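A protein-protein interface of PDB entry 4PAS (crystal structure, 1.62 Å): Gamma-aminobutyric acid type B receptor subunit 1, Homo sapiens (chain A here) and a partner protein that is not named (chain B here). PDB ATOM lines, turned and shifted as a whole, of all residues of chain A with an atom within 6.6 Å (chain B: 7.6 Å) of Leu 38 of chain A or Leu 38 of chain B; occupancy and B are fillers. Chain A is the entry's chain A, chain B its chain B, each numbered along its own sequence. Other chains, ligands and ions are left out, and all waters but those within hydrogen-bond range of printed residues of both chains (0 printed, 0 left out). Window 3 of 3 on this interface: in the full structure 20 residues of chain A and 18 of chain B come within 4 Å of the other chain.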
ATOM      1  N   GLU A  33     -28.901 -23.304  30.452  1.00  0.00           N
ATOM      2  CA  GLU A  33     -28.357 -24.654  30.312  1.00  0.00           C
ATOM      3  C   GLU A  33     -26.929 -24.599  29.798  1.00  0.00           C
ATOM      4  O   GLU A  33     -26.064 -25.340  30.269  1.00  0.00           O
ATOM      5  CB  GLU A  33     -29.220 -25.484  29.357  1.00  0.00           C
ATOM      6  CG  GLU A  33     -30.599 -25.809  29.906  1.00  0.00           C
ATOM      7  CD  GLU A  33     -31.463 -26.592  28.932  1.00  0.00           C
ATOM      8  OE1 GLU A  33     -31.111 -26.669  27.733  1.00  0.00           O
ATOM      9  OE2 GLU A  33     -32.502 -27.128  29.370  1.00  0.00           O
ATOM     10  N   LEU A  34     -26.685 -23.711  28.835  1.00  0.00           N
ATOM     11  CA  LEU A  34     -25.357 -23.559  28.249  1.00  0.00           C
ATOM     12  C   LEU A  34     -24.374 -23.001  29.276  1.00  0.00           C
ATOM     13  O   LEU A  34     -23.214 -23.414  29.337  1.00  0.00           O
ATOM     14  CB  LEU A  34     -25.415 -22.656  27.016  1.00  0.00           C
ATOM     15  CG  LEU A  34     -26.223 -23.195  25.828  1.00  0.00           C
ATOM     16  CD1 LEU A  34     -26.349 -22.133  24.744  1.00  0.00           C
ATOM     17  CD2 LEU A  34     -25.573 -24.455  25.272  1.00  0.00           C
ATOM     18  N   ARG A  35     -24.841 -22.071  30.099  1.00  0.00           N
ATOM     19  CA  ARG A  35     -23.970 -21.497  31.127  1.00  0.00           C
ATOM     20  C   ARG A  35     -23.655 -22.521  32.212  1.00  0.00           C
ATOM     21  O   ARG A  35     -22.558 -22.516  32.774  1.00  0.00           O
ATOM     22  CB  ARG A  35     -24.584 -20.210  31.698  1.00  0.00           C
ATOM     23  CG  ARG A  35     -24.479 -19.066  30.688  1.00  0.00           C
ATOM     24  CD  ARG A  35     -25.126 -17.765  31.121  1.00  0.00           C
ATOM     25  NE  ARG A  35     -24.686 -16.669  30.250  1.00  0.00           N
ATOM     26  CZ  ARG A  35     -25.326 -15.514  30.094  1.00  0.00           C
ATOM     27  NH1 ARG A  35     -26.462 -15.272  30.734  1.00  0.00           N
ATOM     28  NH2 ARG A  35     -24.827 -14.592  29.280  1.00  0.00           N
ATOM     29  N   HIS A  36     -24.600 -23.417  32.484  1.00  0.00           N
ATOM     30  CA  HIS A  36     -24.368 -24.503  33.434  1.00  0.00           C
ATOM     31  C   HIS A  36     -23.266 -25.420  32.896  1.00  0.00           C
ATOM     32  O   HIS A  36     -22.474 -25.979  33.661  1.00  0.00           O
ATOM     33  CB  HIS A  36     -25.656 -25.293  33.677  1.00  0.00           C
ATOM     34  CG  HIS A  36     -25.479 -26.466  34.594  1.00  0.00           C
ATOM     35  ND1 HIS A  36     -25.090 -26.329  35.908  1.00  0.00           N
ATOM     36  CD2 HIS A  36     -25.630 -27.795  34.385  1.00  0.00           C
ATOM     37  CE1 HIS A  36     -25.006 -27.522  36.470  1.00  0.00           C
ATOM     38  NE2 HIS A  36     -25.332 -28.429  35.567  1.00  0.00           N
ATOM     39  N   GLN A  37     -23.209 -25.558  31.573  1.00  0.00           N
ATOM     40  CA  GLN A  37     -22.194 -26.403  30.941  1.00  0.00           C
ATOM     41  C   GLN A  37     -20.798 -25.786  30.968  1.00  0.00           C
ATOM     42  O   GLN A  37     -19.805 -26.502  30.825  1.00  0.00           O
ATOM     43  CB  GLN A  37     -22.588 -26.734  29.505  1.00  0.00           C
ATOM     44  CG  GLN A  37     -23.791 -27.648  29.388  1.00  0.00           C
ATOM     45  CD  GLN A  37     -24.250 -27.762  27.962  1.00  0.00           C
ATOM     46  OE1 GLN A  37     -23.465 -27.537  27.047  1.00  0.00           O
ATOM     47  NE2 GLN A  37     -25.517 -28.103  27.755  1.00  0.00           N
ATOM     48  N   LEU A  38     -20.716 -24.467  31.142  1.00  0.00           N
ATOM     49  CA  LEU A  38     -19.418 -23.795  31.249  1.00  0.00           C
ATOM     50  C   LEU A  38     -18.658 -24.287  32.472  1.00  0.00           C
ATOM     51  O   LEU A  38     -17.456 -24.523  32.403  1.00  0.00           O
ATOM     52  CB  LEU A  38     -19.574 -22.275  31.341  1.00  0.00           C
ATOM     53  CG  LEU A  38     -19.867 -21.448  30.093  1.00  0.00           C
ATOM     54  CD1 LEU A  38     -20.212 -20.020  30.511  1.00  0.00           C
ATOM     55  CD2 LEU A  38     -18.674 -21.467  29.141  1.00  0.00           C
ATOM     56  N   GLN A  39     -19.370 -24.424  33.589  1.00  0.00           N
ATOM     57  CA  GLN A  39     -18.769 -24.870  34.844  1.00  0.00           C
ATOM     58  C   GLN A  39     -18.308 -26.314  34.712  1.00  0.00           C
ATOM     59  O   GLN A  39     -17.111 -26.589  34.609  1.00  0.00           O
ATOM     60  CB  GLN A  39     -19.770 -24.788  35.992  1.00  0.00           C
ATOM     61  CG  GLN A  39     -20.689 -23.590  35.979  1.00  0.00           C
ATOM     62  CD  GLN A  39     -21.754 -23.705  37.043  1.00  0.00           C
ATOM     63  OE1 GLN A  39     -22.512 -24.676  37.079  1.00  0.00           O
ATOM     64  NE2 GLN A  39     -21.813 -22.721  37.928  1.00  0.00           N
ATOM     65  N   SER A  40     -19.275 -27.231  34.713  1.00  0.00           N
ATOM     66  CA  SER A  40     -19.002 -28.662  34.621  1.00  0.00           C
ATOM     67  C   SER A  40     -18.376 -29.031  33.279  1.00  0.00           C
ATOM     68  O   SER A  40     -17.178 -29.350  33.233  1.00  0.00           O
ATOM     69  CB  SER A  40     -20.291 -29.461  34.843  1.00  0.00           C
ATOM     70  OG  SER A  40     -21.289 -29.094  33.906  1.00  0.00           O
ATOM     71  N   GLU B  32     -25.893 -17.409  20.654  1.00  0.00           N
ATOM     72  CA  GLU B  32     -24.710 -17.541  19.814  1.00  0.00           C
ATOM     73  C   GLU B  32     -23.426 -17.285  20.600  1.00  0.00           C
ATOM     74  O   GLU B  32     -22.469 -18.061  20.506  1.00  0.00           O
ATOM     75  CB  GLU B  32     -24.773 -16.601  18.616  1.00  0.00           C
ATOM     76  CG  GLU B  32     -23.708 -16.929  17.576  1.00  0.00           C
ATOM     77  CD  GLU B  32     -23.734 -15.999  16.385  1.00  0.00           C
ATOM     78  OE1 GLU B  32     -23.556 -14.778  16.578  1.00  0.00           O
ATOM     79  OE2 GLU B  32     -23.923 -16.495  15.254  1.00  0.00           O
ATOM     80  N   GLU B  33     -23.416 -16.207  21.378  1.00  0.00           N
ATOM     81  CA  GLU B  33     -22.213 -15.823  22.123  1.00  0.00           C
ATOM     82  C   GLU B  33     -21.808 -16.853  23.170  1.00  0.00           C
ATOM     83  O   GLU B  33     -20.619 -17.146  23.316  1.00  0.00           O
ATOM     84  CB  GLU B  33     -22.368 -14.426  22.738  1.00  0.00           C
ATOM     85  CG  GLU B  33     -22.552 -13.334  21.676  1.00  0.00           C
ATOM     86  CD  GLU B  33     -22.276 -11.920  22.174  1.00  0.00           C
ATOM     87  OE1 GLU B  33     -22.381 -11.667  23.393  1.00  0.00           O
ATOM     88  OE2 GLU B  33     -21.968 -11.054  21.324  1.00  0.00           O
ATOM     89  N   VAL B  34     -22.781 -17.417  23.881  1.00  0.00           N
ATOM     90  CA  VAL B  34     -22.482 -18.451  24.872  1.00  0.00           C
ATOM     91  C   VAL B  34     -22.101 -19.761  24.179  1.00  0.00           C
ATOM     92  O   VAL B  34     -21.224 -20.486  24.651  1.00  0.00           O
ATOM     93  CB  VAL B  34     -23.644 -18.667  25.873  1.00  0.00           C
ATOM     94  CG1 VAL B  34     -23.253 -19.705  26.925  1.00  0.00           C
ATOM     95  CG2 VAL B  34     -23.979 -17.343  26.566  1.00  0.00           C
ATOM     96  N   THR B  35     -22.745 -20.061  23.052  1.00  0.00           N
ATOM     97  CA  THR B  35     -22.393 -21.258  22.295  1.00  0.00           C
ATOM     98  C   THR B  35     -20.942 -21.163  21.827  1.00  0.00           C
ATOM     99  O   THR B  35     -20.209 -22.147  21.882  1.00  0.00           O
ATOM    100  CB  THR B  35     -23.326 -21.471  21.078  1.00  0.00           C
ATOM    101  OG1 THR B  35     -24.643 -21.785  21.540  1.00  0.00           O
ATOM    102  CG2 THR B  35     -22.831 -22.617  20.210  1.00  0.00           C
ATOM    103  N   MET B  36     -20.529 -19.977  21.382  1.00  0.00           N
ATOM    104  CA  MET B  36     -19.140 -19.769  20.941  1.00  0.00           C
ATOM    105  C   MET B  36     -18.172 -19.883  22.123  1.00  0.00           C
ATOM    106  O   MET B  36     -17.077 -20.436  21.996  1.00  0.00           O
ATOM    107  CB  MET B  36     -18.983 -18.408  20.254  1.00  0.00           C
ATOM    108  CG  MET B  36     -19.742 -18.275  18.936  1.00  0.00           C
ATOM    109  SD  MET B  36     -19.396 -16.741  18.043  1.00  0.00           S
ATOM    110  CE  MET B  36     -18.183 -17.310  16.852  1.00  0.00           C
ATOM    111  N   GLN B  37     -18.592 -19.374  23.277  1.00  0.00           N
ATOM    112  CA  GLN B  37     -17.786 -19.436  24.494  1.00  0.00           C
ATOM    113  C   GLN B  37     -17.578 -20.880  24.947  1.00  0.00           C
ATOM    114  O   GLN B  37     -16.482 -21.261  25.370  1.00  0.00           O
ATOM    115  CB  GLN B  37     -18.465 -18.629  25.611  1.00  0.00           C
ATOM    116  CG  GLN B  37     -17.613 -18.468  26.866  1.00  0.00           C
ATOM    117  CD  GLN B  37     -18.298 -17.651  27.954  1.00  0.00           C
ATOM    118  OE1 GLN B  37     -19.437 -17.199  27.796  1.00  0.00           O
ATOM    119  NE2 GLN B  37     -17.603 -17.467  29.070  1.00  0.00           N
ATOM    120  N   LEU B  38     -18.637 -21.677  24.843  1.00  0.00           N
ATOM    121  CA  LEU B  38     -18.634 -23.068  25.292  1.00  0.00           C
ATOM    122  C   LEU B  38     -17.869 -24.004  24.351  1.00  0.00           C
ATOM    123  O   LEU B  38     -17.215 -24.948  24.798  1.00  0.00           O
ATOM    124  CB  LEU B  38     -20.080 -23.549  25.461  1.00  0.00           C
ATOM    125  CG  LEU B  38     -20.366 -24.892  26.130  1.00  0.00           C
ATOM    126  CD1 LEU B  38     -19.832 -24.911  27.558  1.00  0.00           C
ATOM    127  CD2 LEU B  38     -21.866 -25.146  26.119  1.00  0.00           C
ATOM    128  N   GLN B  39     -17.946 -23.735  23.053  1.00  0.00           N
ATOM    129  CA  GLN B  39     -17.299 -24.579  22.053  1.00  0.00           C
ATOM    130  C   GLN B  39     -15.865 -24.140  21.762  1.00  0.00           C
ATOM    131  O   GLN B  39     -15.457 -23.026  22.134  1.00  0.00           O
ATOM    132  CB  GLN B  39     -18.130 -24.610  20.764  1.00  0.00           C
ATOM    133  CG  GLN B  39     -19.504 -25.268  20.939  1.00  0.00           C
ATOM    134  CD  GLN B  39     -20.356 -25.262  19.676  1.00  0.00           C
ATOM    135  OE1 GLN B  39     -19.908 -24.861  18.600  1.00  0.00           O
ATOM    136  NE2 GLN B  39     -21.597 -25.713  19.807  1.00  0.00           N
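Printed residues of chain B within 4 Å of Leu 34 of chain A: Val 34 (3.7 Å), Thr 35 (3.6 Å) and Leu 38 (3.9 Å). Of the printed residues of chain B, Arg 35 of chain A touches Val 34 (3.8 Å). Of the printed residues of chain B, Leu 38 of chain A touches Gln 37 and Leu 38. Gln 39 of chain A touches none of the printed residues of chain B. Of the printed residues of chain A, Val 34 of chain B touches Leu 34 and Arg 35. Printed residues of chain A within 4 Å of Gln 37 of chain B: Leu 38. Leu 38 of chain B touches just these residues of chain A: Leu 34 (3.9 Å), Gln 37 (3.0 Å) and Leu 38 (3.7 Å). Gln 39 of chain B touches none of the printed residues of chain A. The nearest residue of chain A that does not touch Leu 38 of chain B is Arg 35 of chain A (5.8 Å). The nearest printed residue of chain B that does not touch Arg 35 of chain A is Gln 37 of chain B (5.8 Å).
Among the printed residues, pairs that only touch across the chains: Leu 34 of chain A with Val 34 of chain B (3.7 Å), Leu 34 of chain A with Thr 35 of chain B (3.6 Å), Leu 34 of chain A with Leu 38 of chain B (3.9 Å), Arg 35 of chain A with Val 34 of chain B (3.8 Å), Gln 37 of chain A with Leu 38 of chain B (3.0 Å), Leu 38 of chain A with Gln 37 of chain B (3.9 Å) and Leu 38 of chain A with Leu 38 of chain B (3.7 Å).
Hydrophobic or aromatic side chains of chain B that line the printed part of chain A: Val 34 and Leu 38. Along chain B the printed residues that touch a printed residue of chain A span positions 34 to 38. Of the 8 printed residues of chain A, 4 touch a printed residue of chain B. Hydrophobic or aromatic side chains of chain A within 4 Å of the printed part of chain B: Leu 34 and Leu 38.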
